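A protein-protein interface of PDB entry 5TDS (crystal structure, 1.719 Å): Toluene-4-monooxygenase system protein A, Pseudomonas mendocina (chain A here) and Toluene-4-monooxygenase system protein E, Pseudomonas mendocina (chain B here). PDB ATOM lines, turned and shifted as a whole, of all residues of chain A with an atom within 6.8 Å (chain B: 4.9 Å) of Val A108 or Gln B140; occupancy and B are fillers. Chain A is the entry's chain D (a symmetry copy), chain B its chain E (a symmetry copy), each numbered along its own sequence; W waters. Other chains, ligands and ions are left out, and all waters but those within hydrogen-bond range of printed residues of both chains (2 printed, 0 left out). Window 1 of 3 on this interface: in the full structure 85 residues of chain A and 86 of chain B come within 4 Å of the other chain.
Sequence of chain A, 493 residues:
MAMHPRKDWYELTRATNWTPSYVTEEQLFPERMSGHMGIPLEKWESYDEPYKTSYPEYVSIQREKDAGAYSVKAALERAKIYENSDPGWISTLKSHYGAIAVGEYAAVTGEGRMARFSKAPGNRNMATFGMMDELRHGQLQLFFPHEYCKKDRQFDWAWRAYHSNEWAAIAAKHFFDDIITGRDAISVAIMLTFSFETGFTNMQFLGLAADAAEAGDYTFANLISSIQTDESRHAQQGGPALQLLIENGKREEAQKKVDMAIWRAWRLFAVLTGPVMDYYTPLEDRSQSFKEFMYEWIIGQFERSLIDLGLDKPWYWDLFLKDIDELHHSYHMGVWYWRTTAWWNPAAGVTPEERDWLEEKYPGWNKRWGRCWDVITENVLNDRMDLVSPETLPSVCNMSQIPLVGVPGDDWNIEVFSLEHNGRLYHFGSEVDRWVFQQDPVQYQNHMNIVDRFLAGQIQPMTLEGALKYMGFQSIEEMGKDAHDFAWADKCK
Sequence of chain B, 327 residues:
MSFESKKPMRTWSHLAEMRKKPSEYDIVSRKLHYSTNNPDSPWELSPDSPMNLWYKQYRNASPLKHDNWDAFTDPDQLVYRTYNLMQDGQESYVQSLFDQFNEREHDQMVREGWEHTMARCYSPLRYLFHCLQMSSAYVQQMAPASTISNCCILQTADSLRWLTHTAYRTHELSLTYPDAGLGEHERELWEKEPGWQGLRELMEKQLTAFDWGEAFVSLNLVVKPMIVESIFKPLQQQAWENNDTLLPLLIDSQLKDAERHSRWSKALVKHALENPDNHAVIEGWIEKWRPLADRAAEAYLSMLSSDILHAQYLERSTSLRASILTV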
ATOM      1  N   GLY A 103      -1.707  18.635  23.628  1.00  0.00           N
ATOM      2  CA  GLY A 103      -2.612  19.627  23.067  1.00  0.00           C
ATOM      3  C   GLY A 103      -3.866  18.983  22.493  1.00  0.00           C
ATOM      4  O   GLY A 103      -4.975  19.513  22.632  1.00  0.00           O
ATOM      5  N   GLU A 104      -3.704  17.849  21.822  1.00  0.00           N
ATOM      6  CA  GLU A 104      -4.867  17.089  21.369  1.00  0.00           C
ATOM      7  C   GLU A 104      -5.762  16.757  22.551  1.00  0.00           C
ATOM      8  O   GLU A 104      -6.982  16.891  22.480  1.00  0.00           O
ATOM      9  CB  GLU A 104      -4.445  15.804  20.666  1.00  0.00           C
ATOM     10  CG  GLU A 104      -3.642  16.044  19.401  1.00  0.00           C
ATOM     11  CD  GLU A 104      -4.466  15.833  18.153  1.00  0.00           C
ATOM     12  OE1 GLU A 104      -5.696  16.020  18.237  1.00  0.00           O
ATOM     13  OE2 GLU A 104      -3.884  15.486  17.103  1.00  0.00           O
ATOM     14  N   TYR A 105      -5.152  16.327  23.651  1.00  0.00           N
ATOM     15  CA  TYR A 105      -5.954  15.995  24.809  1.00  0.00           C
ATOM     16  C   TYR A 105      -6.649  17.254  25.337  1.00  0.00           C
ATOM     17  O   TYR A 105      -7.791  17.189  25.791  1.00  0.00           O
ATOM     18  CB  TYR A 105      -5.112  15.326  25.908  1.00  0.00           C
ATOM     19  CG  TYR A 105      -5.975  14.881  27.063  1.00  0.00           C
ATOM     20  CD1 TYR A 105      -6.817  13.777  26.944  1.00  0.00           C
ATOM     21  CD2 TYR A 105      -5.978  15.585  28.264  1.00  0.00           C
ATOM     22  CE1 TYR A 105      -7.636  13.388  27.991  1.00  0.00           C
ATOM     23  CE2 TYR A 105      -6.780  15.191  29.320  1.00  0.00           C
ATOM     24  CZ  TYR A 105      -7.604  14.101  29.180  1.00  0.00           C
ATOM     25  OH  TYR A 105      -8.415  13.742  30.226  1.00  0.00           O
ATOM     26  N   ALA A 106      -5.967  18.395  25.289  1.00  0.00           N
ATOM     27  CA  ALA A 106      -6.587  19.658  25.685  1.00  0.00           C
ATOM     28  C   ALA A 106      -7.798  19.979  24.813  1.00  0.00           C
ATOM     29  O   ALA A 106      -8.764  20.584  25.278  1.00  0.00           O
ATOM     30  CB  ALA A 106      -5.573  20.808  25.624  1.00  0.00           C
ATOM     31  N   ALA A 107      -7.757  19.567  23.548  1.00  0.00           N
ATOM     32  CA  ALA A 107      -8.884  19.822  22.661  1.00  0.00           C
ATOM     33  C   ALA A 107     -10.147  19.105  23.137  1.00  0.00           C
ATOM     34  O   ALA A 107     -11.242  19.485  22.751  1.00  0.00           O
ATOM     35  CB  ALA A 107      -8.548  19.399  21.222  1.00  0.00           C
ATOM     36  N   VAL A 108     -10.008  18.046  23.935  1.00  0.00           N
ATOM     37  CA  VAL A 108     -11.199  17.401  24.504  1.00  0.00           C
ATOM     38  C   VAL A 108     -12.035  18.448  25.252  1.00  0.00           C
ATOM     39  O   VAL A 108     -13.270  18.469  25.181  1.00  0.00           O
ATOM     40  CB  VAL A 108     -10.849  16.244  25.477  1.00  0.00           C
ATOM     41  CG1 VAL A 108     -12.116  15.698  26.130  1.00  0.00           C
ATOM     42  CG2 VAL A 108     -10.091  15.112  24.746  1.00  0.00           C
ATOM     43  N   THR A 109     -11.341  19.335  25.946  1.00  0.00           N
ATOM     44  CA  THR A 109     -11.976  20.364  26.769  1.00  0.00           C
ATOM     45  C   THR A 109     -12.659  21.448  25.925  1.00  0.00           C
ATOM     46  O   THR A 109     -13.724  21.952  26.286  1.00  0.00           O
ATOM     47  CB  THR A 109     -10.938  20.975  27.707  1.00  0.00           C
ATOM     48  OG1 THR A 109     -10.627  20.006  28.708  1.00  0.00           O
ATOM     49  CG2 THR A 109     -11.450  22.273  28.372  1.00  0.00           C
ATOM     50  N   GLY A 110     -12.058  21.794  24.795  1.00  0.00           N
ATOM     51  CA  GLY A 110     -12.717  22.690  23.852  1.00  0.00           C
ATOM     52  C   GLY A 110     -14.012  22.070  23.348  1.00  0.00           C
ATOM     53  O   GLY A 110     -15.062  22.723  23.284  1.00  0.00           O
ATOM     54  N   GLU A 111     -13.947  20.793  22.990  1.00  0.00           N
ATOM     55  CA  GLU A 111     -15.144  20.097  22.531  1.00  0.00           C
ATOM     56  C   GLU A 111     -16.160  19.960  23.686  1.00  0.00           C
ATOM     57  O   GLU A 111     -17.364  20.145  23.494  1.00  0.00           O
ATOM     58  CB  GLU A 111     -14.758  18.736  21.940  1.00  0.00           C
ATOM     59  CG  GLU A 111     -13.884  18.838  20.675  1.00  0.00           C
ATOM     60  CD  GLU A 111     -14.674  19.252  19.430  1.00  0.00           C
ATOM     61  OE1 GLU A 111     -15.922  19.213  19.481  1.00  0.00           O
ATOM     62  OE2 GLU A 111     -14.044  19.608  18.402  1.00  0.00           O
ATOM     63  N   GLY A 112     -15.679  19.659  24.891  1.00  0.00           N
ATOM     64  CA  GLY A 112     -16.557  19.581  26.051  1.00  0.00           C
ATOM     65  C   GLY A 112     -17.244  20.902  26.372  1.00  0.00           C
ATOM     66  O   GLY A 112     -18.406  20.933  26.805  1.00  0.00           O
ATOM     67  N   ARG A 113     -16.532  22.001  26.150  1.00  0.00           N
ATOM     68  CA  ARG A 113     -17.119  23.327  26.347  1.00  0.00           C
ATOM     69  C   ARG A 113     -18.348  23.506  25.456  1.00  0.00           C
ATOM     70  O   ARG A 113     -19.371  24.056  25.890  1.00  0.00           O
ATOM     71  CB  ARG A 113     -16.088  24.426  26.059  1.00  0.00           C
ATOM     72  CG  ARG A 113     -16.464  25.792  26.614  1.00  0.00           C
ATOM     73  CD  ARG A 113     -16.020  25.919  28.075  1.00  0.00           C
ATOM     74  NE  ARG A 113     -14.564  25.869  28.216  1.00  0.00           N
ATOM     75  CZ  ARG A 113     -13.924  25.294  29.235  1.00  0.00           C
ATOM     76  NH1 ARG A 113     -14.592  24.692  30.208  1.00  0.00           N
ATOM     77  NH2 ARG A 113     -12.604  25.307  29.280  1.00  0.00           N
ATOM     78  N   ALA A 127     -20.074  17.814  19.190  1.00  0.00           N
ATOM     79  CA  ALA A 127     -18.982  18.090  20.126  1.00  0.00           C
ATOM     80  C   ALA A 127     -18.734  16.896  21.030  1.00  0.00           C
ATOM     81  O   ALA A 127     -17.637  16.715  21.556  1.00  0.00           O
ATOM     82  CB  ALA A 127     -19.294  19.353  20.974  1.00  0.00           C
ATOM     83  N   GLY A 130     -16.635  14.868  19.093  1.00  0.00           N
ATOM     84  CA  GLY A 130     -15.369  15.582  19.108  1.00  0.00           C
ATOM     85  C   GLY A 130     -14.564  15.304  20.368  1.00  0.00           C
ATOM     86  O   GLY A 130     -13.342  15.170  20.295  1.00  0.00           O
ATOM     87  N   MET A 131     -15.236  15.219  21.517  1.00  0.00           N
ATOM     88  CA  MET A 131     -14.551  14.848  22.767  1.00  0.00           C
ATOM     89  C   MET A 131     -13.893  13.489  22.602  1.00  0.00           C
ATOM     90  O   MET A 131     -12.739  13.281  23.001  1.00  0.00           O
ATOM     91  CB  MET A 131     -15.523  14.808  23.951  1.00  0.00           C
ATOM     92  CG  MET A 131     -16.048  16.164  24.363  1.00  0.00           C
ATOM     93  SD  MET A 131     -17.490  15.984  25.459  1.00  0.00           S
ATOM     94  CE  MET A 131     -16.708  15.470  26.988  1.00  0.00           C
ATOM     95  N   MET A 132     -14.641  12.564  22.014  1.00  0.00           N
ATOM     96  CA  MET A 132     -14.134  11.223  21.799  1.00  0.00           C
ATOM     97  C   MET A 132     -12.973  11.207  20.805  1.00  0.00           C
ATOM     98  O   MET A 132     -11.958  10.537  21.041  1.00  0.00           O
ATOM     99  CB  MET A 132     -15.275  10.301  21.331  1.00  0.00           C
ATOM    100  CG  MET A 132     -16.274   9.982  22.448  1.00  0.00           C
ATOM    101  SD  MET A 132     -15.567   8.888  23.710  1.00  0.00           S
ATOM    102  CE  MET A 132     -15.700   7.296  22.887  1.00  0.00           C
ATOM    103  N   ASP A 133     -13.107  11.941  19.700  1.00  0.00           N
ATOM    104  CA  ASP A 133     -12.041  11.984  18.705  1.00  0.00           C
ATOM    105  C   ASP A 133     -10.733  12.492  19.300  1.00  0.00           C
ATOM    106  O   ASP A 133      -9.674  11.918  19.052  1.00  0.00           O
ATOM    107  CB  ASP A 133     -12.413  12.872  17.521  1.00  0.00           C
ATOM    108  CG  ASP A 133     -13.470  12.250  16.625  1.00  0.00           C
ATOM    109  OD1 ASP A 133     -13.751  11.045  16.757  1.00  0.00           O
ATOM    110  OD2 ASP A 133     -14.001  12.977  15.766  1.00  0.00           O
ATOM    111  N   GLU A 134     -10.798  13.576  20.070  1.00  0.00           N
ATOM    112  CA  GLU A 134      -9.565  14.170  20.571  1.00  0.00           C
ATOM    113  C   GLU A 134      -8.982  13.312  21.691  1.00  0.00           C
ATOM    114  O   GLU A 134      -7.762  13.287  21.875  1.00  0.00           O
ATOM    115  CB  GLU A 134      -9.801  15.611  21.032  1.00  0.00           C
ATOM    116  CG  GLU A 134     -10.423  16.505  19.957  1.00  0.00           C
ATOM    117  CD  GLU A 134      -9.545  16.714  18.733  1.00  0.00           C
ATOM    118  OE1 GLU A 134      -8.547  15.988  18.562  1.00  0.00           O
ATOM    119  OE2 GLU A 134      -9.859  17.631  17.953  1.00  0.00           O
ATOM    120  N   LEU A 135      -9.839  12.598  22.425  1.00  0.00           N
ATOM    121  CA  LEU A 135      -9.352  11.603  23.384  1.00  0.00           C
ATOM    122  C   LEU A 135      -8.511  10.552  22.659  1.00  0.00           C
ATOM    123  O   LEU A 135      -7.391  10.227  23.078  1.00  0.00           O
ATOM    124  CB  LEU A 135     -10.516  10.934  24.125  1.00  0.00           C
ATOM    125  CG  LEU A 135     -10.127   9.821  25.110  1.00  0.00           C
ATOM    126  CD1 LEU A 135      -9.301  10.394  26.273  1.00  0.00           C
ATOM    127  CD2 LEU A 135     -11.373   9.109  25.629  1.00  0.00           C
ATOM    128  N   ARG A 136      -9.050  10.030  21.563  1.00  0.00           N
ATOM    129  CA  ARG A 136      -8.292   9.115  20.713  1.00  0.00           C
ATOM    130  C   ARG A 136      -6.938   9.704  20.327  1.00  0.00           C
ATOM    131  O   ARG A 136      -5.896   9.046  20.442  1.00  0.00           O
ATOM    132  CB  ARG A 136      -9.074   8.782  19.442  1.00  0.00           C
ATOM    133  CG  ARG A 136      -8.352   7.763  18.558  1.00  0.00           C
ATOM    134  CD  ARG A 136      -8.992   7.554  17.198  1.00  0.00           C
ATOM    135  NE  ARG A 136      -8.273   6.467  16.526  1.00  0.00           N
ATOM    136  CZ  ARG A 136      -7.857   6.485  15.264  1.00  0.00           C
ATOM    137  NH1 ARG A 136      -8.137   7.515  14.468  1.00  0.00           N
ATOM    138  NH2 ARG A 136      -7.184   5.442  14.790  1.00  0.00           N
ATOM    139  N   GLY A 138      -5.116  12.201  21.531  1.00  0.00           N
ATOM    140  CA  GLY A 138      -4.200  12.373  22.645  1.00  0.00           C
ATOM    141  C   GLY A 138      -3.609  11.044  23.080  1.00  0.00           C
ATOM    142  O   GLY A 138      -2.399  10.929  23.301  1.00  0.00           O
ATOM    143  N   ILE A 180      -8.802  27.188  22.340  1.00  0.00           N
ATOM    144  CA  ILE A 180      -9.430  25.911  22.695  1.00  0.00           C
ATOM    145  C   ILE A 180     -10.058  25.903  24.085  1.00  0.00           C
ATOM    146  O   ILE A 180     -11.262  25.645  24.253  1.00  0.00           O
ATOM    147  CB  ILE A 180      -8.414  24.738  22.646  1.00  0.00           C
ATOM    148  CG1 ILE A 180      -7.822  24.592  21.247  1.00  0.00           C
ATOM    149  CG2 ILE A 180      -9.100  23.429  23.021  1.00  0.00           C
ATOM    150  CD1 ILE A 180      -6.956  23.344  21.077  1.00  0.00           C
ATOM    151  N   THR A 181      -9.236  26.173  25.089  1.00  0.00           N
ATOM    152  CA  THR A 181      -9.663  25.981  26.468  1.00  0.00           C
ATOM    153  C   THR A 181     -10.075  27.248  27.208  1.00  0.00           C
ATOM    154  O   THR A 181     -10.647  27.158  28.289  1.00  0.00           O
ATOM    155  CB  THR A 181      -8.551  25.321  27.290  1.00  0.00           C
ATOM    156  OG1 THR A 181      -7.356  26.091  27.154  1.00  0.00           O
ATOM    157  CG2 THR A 181      -8.288  23.899  26.792  1.00  0.00           C
ATOM    158  N   LEU A 192     -11.272  27.187  16.881  1.00  0.00           N
ATOM    159  CA  LEU A 192     -10.658  25.867  16.826  1.00  0.00           C
ATOM    160  C   LEU A 192     -11.132  25.072  15.613  1.00  0.00           C
ATOM    161  O   LEU A 192     -10.312  24.662  14.793  1.00  0.00           O
ATOM    162  CB  LEU A 192     -10.924  25.072  18.106  1.00  0.00           C
ATOM    163  CG  LEU A 192     -10.585  23.561  18.048  1.00  0.00           C
ATOM    164  CD1 LEU A 192      -9.088  23.315  17.825  1.00  0.00           C
ATOM    165  CD2 LEU A 192     -11.068  22.832  19.311  1.00  0.00           C
ATOM    166  N   HIS B  33      -3.667  16.977  32.694  1.00  0.00           N
ATOM    167  CA  HIS B  33      -4.186  18.332  32.888  1.00  0.00           C
ATOM    168  C   HIS B  33      -3.088  19.288  33.338  1.00  0.00           C
ATOM    169  O   HIS B  33      -2.951  19.550  34.540  1.00  0.00           O
ATOM    170  CB  HIS B  33      -5.308  18.362  33.944  1.00  0.00           C
ATOM    171  CG  HIS B  33      -6.627  17.806  33.487  1.00  0.00           C
ATOM    172  ND1 HIS B  33      -6.958  17.622  32.162  1.00  0.00           N
ATOM    173  CD2 HIS B  33      -7.708  17.409  34.205  1.00  0.00           C
ATOM    174  CE1 HIS B  33      -8.183  17.125  32.081  1.00  0.00           C
ATOM    175  NE2 HIS B  33      -8.662  16.992  33.307  1.00  0.00           N
ATOM    176  N   SER B 136     -22.483  15.513  32.131  1.00  0.00           N
ATOM    177  CA  SER B 136     -21.262  14.719  32.102  1.00  0.00           C
ATOM    178  C   SER B 136     -20.125  15.483  31.419  1.00  0.00           C
ATOM    179  O   SER B 136     -18.989  15.438  31.874  1.00  0.00           O
ATOM    180  CB  SER B 136     -21.498  13.380  31.394  1.00  0.00           C
ATOM    181  OG  SER B 136     -22.513  12.643  32.048  1.00  0.00           O
ATOM    182  N   ALA B 137     -20.434  16.194  30.340  1.00  0.00           N
ATOM    183  CA  ALA B 137     -19.419  16.987  29.645  1.00  0.00           C
ATOM    184  C   ALA B 137     -18.886  18.084  30.546  1.00  0.00           C
ATOM    185  O   ALA B 137     -17.707  18.443  30.476  1.00  0.00           O
ATOM    186  CB  ALA B 137     -19.986  17.590  28.370  1.00  0.00           C
ATOM    187  N   TYR B 138     -19.750  18.636  31.388  1.00  0.00           N
ATOM    188  CA  TYR B 138     -19.285  19.673  32.301  1.00  0.00           C
ATOM    189  C   TYR B 138     -18.326  19.105  33.346  1.00  0.00           C
ATOM    190  O   TYR B 138     -17.291  19.714  33.643  1.00  0.00           O
ATOM    191  CB  TYR B 138     -20.443  20.382  33.002  1.00  0.00           C
ATOM    192  CG  TYR B 138     -19.915  21.527  33.820  1.00  0.00           C
ATOM    193  CD1 TYR B 138     -19.410  22.664  33.199  1.00  0.00           C
ATOM    194  CD2 TYR B 138     -19.851  21.443  35.203  1.00  0.00           C
ATOM    195  CE1 TYR B 138     -18.893  23.716  33.945  1.00  0.00           C
ATOM    196  CE2 TYR B 138     -19.340  22.484  35.958  1.00  0.00           C
ATOM    197  CZ  TYR B 138     -18.859  23.614  35.322  1.00  0.00           C
ATOM    198  OH  TYR B 138     -18.333  24.648  36.070  1.00  0.00           O
ATOM    199  N   VAL B 139     -18.658  17.957  33.923  1.00  0.00           N
ATOM    200  CA  VAL B 139     -17.737  17.372  34.884  1.00  0.00           C
ATOM    201  C   VAL B 139     -16.411  17.048  34.182  1.00  0.00           C
ATOM    202  O   VAL B 139     -15.343  17.273  34.747  1.00  0.00           O
ATOM    203  CB  VAL B 139     -18.306  16.114  35.561  1.00  0.00           C
ATOM    204  CG1 VAL B 139     -17.361  15.652  36.662  1.00  0.00           C
ATOM    205  CG2 VAL B 139     -19.688  16.413  36.162  1.00  0.00           C
ATOM    206  N   GLN B 140     -16.478  16.541  32.945  1.00  0.00           N
ATOM    207  CA  GLN B 140     -15.259  16.323  32.163  1.00  0.00           C
ATOM    208  C   GLN B 140     -14.352  17.552  32.155  1.00  0.00           C
ATOM    209  O   GLN B 140     -13.170  17.466  32.497  1.00  0.00           O
ATOM    210  CB  GLN B 140     -15.583  15.934  30.706  1.00  0.00           C
ATOM    211  CG  GLN B 140     -14.331  15.851  29.800  1.00  0.00           C
ATOM    212  CD  GLN B 140     -13.916  17.198  29.216  1.00  0.00           C
ATOM    213  OE1 GLN B 140     -14.759  17.986  28.766  1.00  0.00           O
ATOM    214  NE2 GLN B 140     -12.618  17.475  29.235  1.00  0.00           N
ATOM    215  N   GLN B 141     -14.894  18.698  31.754  1.00  0.00           N
ATOM    216  CA  GLN B 141     -14.013  19.831  31.501  1.00  0.00           C
ATOM    217  C   GLN B 141     -13.509  20.453  32.797  1.00  0.00           C
ATOM    218  O   GLN B 141     -12.470  21.116  32.789  1.00  0.00           O
ATOM    219  CB  GLN B 141     -14.713  20.885  30.631  1.00  0.00           C
ATOM    220  CG  GLN B 141     -15.946  21.524  31.279  1.00  0.00           C
ATOM    221  CD  GLN B 141     -16.919  22.077  30.249  1.00  0.00           C
ATOM    222  OE1 GLN B 141     -16.999  23.291  30.033  1.00  0.00           O
ATOM    223  NE2 GLN B 141     -17.669  21.185  29.604  1.00  0.00           N
ATOM    224  N   MET B 142     -14.214  20.225  33.906  1.00  0.00           N
ATOM    225  CA  MET B 142     -13.820  20.841  35.185  1.00  0.00           C
ATOM    226  C   MET B 142     -13.027  19.935  36.139  1.00  0.00           C
ATOM    227  O   MET B 142     -12.400  20.439  37.072  1.00  0.00           O
ATOM    228  CB  MET B 142     -15.052  21.361  35.937  1.00  0.00           C
ATOM    229  CG  MET B 142     -15.853  22.435  35.208  1.00  0.00           C
ATOM    230  SD  MET B 142     -14.866  23.782  34.504  1.00  0.00           S
ATOM    231  CE  MET B 142     -13.968  24.310  35.962  1.00  0.00           C
ATOM    232  N   ALA B 143     -13.060  18.617  35.937  1.00  0.00           N
ATOM    233  CA  ALA B 143     -12.428  17.694  36.891  1.00  0.00           C
ATOM    234  C   ALA B 143     -10.928  17.946  36.985  1.00  0.00           C
ATOM    235  O   ALA B 143     -10.290  18.247  35.984  1.00  0.00           O
ATOM    236  CB  ALA B 143     -12.699  16.243  36.505  1.00  0.00           C
ATOM    237  N   SER B 149     -11.480  12.992  34.373  1.00  0.00           N
ATOM    238  CA  SER B 149     -12.095  13.507  33.149  1.00  0.00           C
ATOM    239  C   SER B 149     -12.362  12.415  32.096  1.00  0.00           C
ATOM    240  O   SER B 149     -13.382  12.464  31.410  1.00  0.00           O
ATOM    241  CB  SER B 149     -11.231  14.603  32.536  1.00  0.00           C
ATOM    242  OG  SER B 149     -11.208  15.755  33.368  1.00  0.00           O
ATOM    243  N   CYS B 152     -15.465  10.667  32.664  1.00  0.00           N
ATOM    244  CA  CYS B 152     -16.563  11.555  32.297  1.00  0.00           C
ATOM    245  C   CYS B 152     -16.796  11.602  30.784  1.00  0.00           C
ATOM    246  O   CYS B 152     -17.942  11.701  30.336  1.00  0.00           O
ATOM    247  CB  CYS B 152     -16.305  12.968  32.816  1.00  0.00           C
ATOM    248  SG  CYS B 152     -16.347  13.057  34.603  1.00  0.00           S
ATOM    249  N   ILE B 153     -15.713  11.561  30.007  1.00  0.00           N
ATOM    250  CA  ILE B 153     -15.842  11.567  28.548  1.00  0.00           C
ATOM    251  C   ILE B 153     -16.655  10.363  28.092  1.00  0.00           C
ATOM    252  O   ILE B 153     -17.586  10.477  27.287  1.00  0.00           O
ATOM    253  CB  ILE B 153     -14.477  11.512  27.828  1.00  0.00           C
ATOM    254  CG1 ILE B 153     -13.626  12.741  28.163  1.00  0.00           C
ATOM    255  CG2 ILE B 153     -14.682  11.356  26.309  1.00  0.00           C
ATOM    256  CD1 ILE B 153     -12.126  12.549  27.787  1.00  0.00           C
HETATM  257  O   HOH W   1     -10.351  21.054  31.231  1.00  0.00           O
HETATM  258  O   HOH W   2     -10.149  15.980  29.587  1.00  0.00           O
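Among the printed residues, pairs that only touch across the chains: Val A108 with Ile B153 (3.6 Å), Val A108 with Gln B140 (3.6 Å), Gly A112 with Gln B140 (3.6 Å), Met A131 with Gln B140 (3.6 Å), Tyr A105 with His B33 (3.7 Å), Met A132 with Ile B153 (3.7 Å), Tyr A105 with Ser B149 (3.7 Å) and Leu A135 with Ile B153 (3.9 Å).
Water W1 lies within hydrogen-bond range of the backbone carbonyl oxygen of Gln B141 (2.6 Å) and the side-chain hydroxyl of Thr A109 (2.7 Å).
Water W2 lies within hydrogen-bond range of OH of Tyr A105 (2.9 Å) and NE2 of Gln B140 (2.9 Å).
Hydrophobic or aromatic side chains of chain B within 4 Å of the printed part of chain A: His B33 and Ile B153.
Of the 23 printed residues of chain A, 8 touch a printed residue of chain B.
Printed residues of chain A that touch a printed residue of chain B: Tyr A105, Val A108, Thr A109, Gly A112, Arg A113, Met A131, Met A132 and Leu A135.
Among the printed residues, no Asp or Glu carboxylate lies within 4 Å of a Lys or Arg side-chain nitrogen of the other chain.
O of Thr A181 is in hydrogen-bond range of NH2 of Arg A113 (2.9 Å).
A ring nitrogen (NE2) of His B33 sits close to the backbone carbonyl oxygen of Ala B143 (3.4 Å).
The backbone carbonyl oxygen (O) of Ala B137 sits at hydrogen-bond distance from the side-chain amide nitrogen (NE2) of Gln B141, at 2.9 Å.
The backbone carbonyl oxygen (O) of Gln B140 sits at hydrogen-bond distance from the side-chain hydroxyl (OG) of Ser B149 (2.7 Å).
The backbone carbonyl oxygen (O) of Ala B137 lies close to the side-chain amide oxygen (OE1) of Gln B140, at 3.4 Å.
A ring nitrogen (NE2) of His B33 lies within hydrogen-bond range of the side-chain hydroxyl (OG) of Ser B149, 2.8 Å away.
The side-chain amide nitrogen (NE2) of Gln B140 lies within hydrogen-bond range of the side-chain hydroxyl (OG1) of Thr A109.
NE2 of Gln B141 sits at hydrogen-bond distance from O of Gly A112 (2.9 Å).
The guanidinium group of Arg A113 sits at hydrogen-bond distance from the side-chain amide oxygen of Gln B141 (2.8 Å).
Val A108 touches just these residues of chain B: Gln B140 and Ile B153.
Of the printed residues of chain A, His B33 touches Tyr A105 (3.7 Å).
Printed residues of chain A within 4 Å of Ile B153: Val A108 (3.6 Å), Met A132 (3.7 Å) and Leu A135 (3.9 Å).
Ala A107 touches none of the printed residues of chain B.
Gly A103 touches none of the printed residues of chain B.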
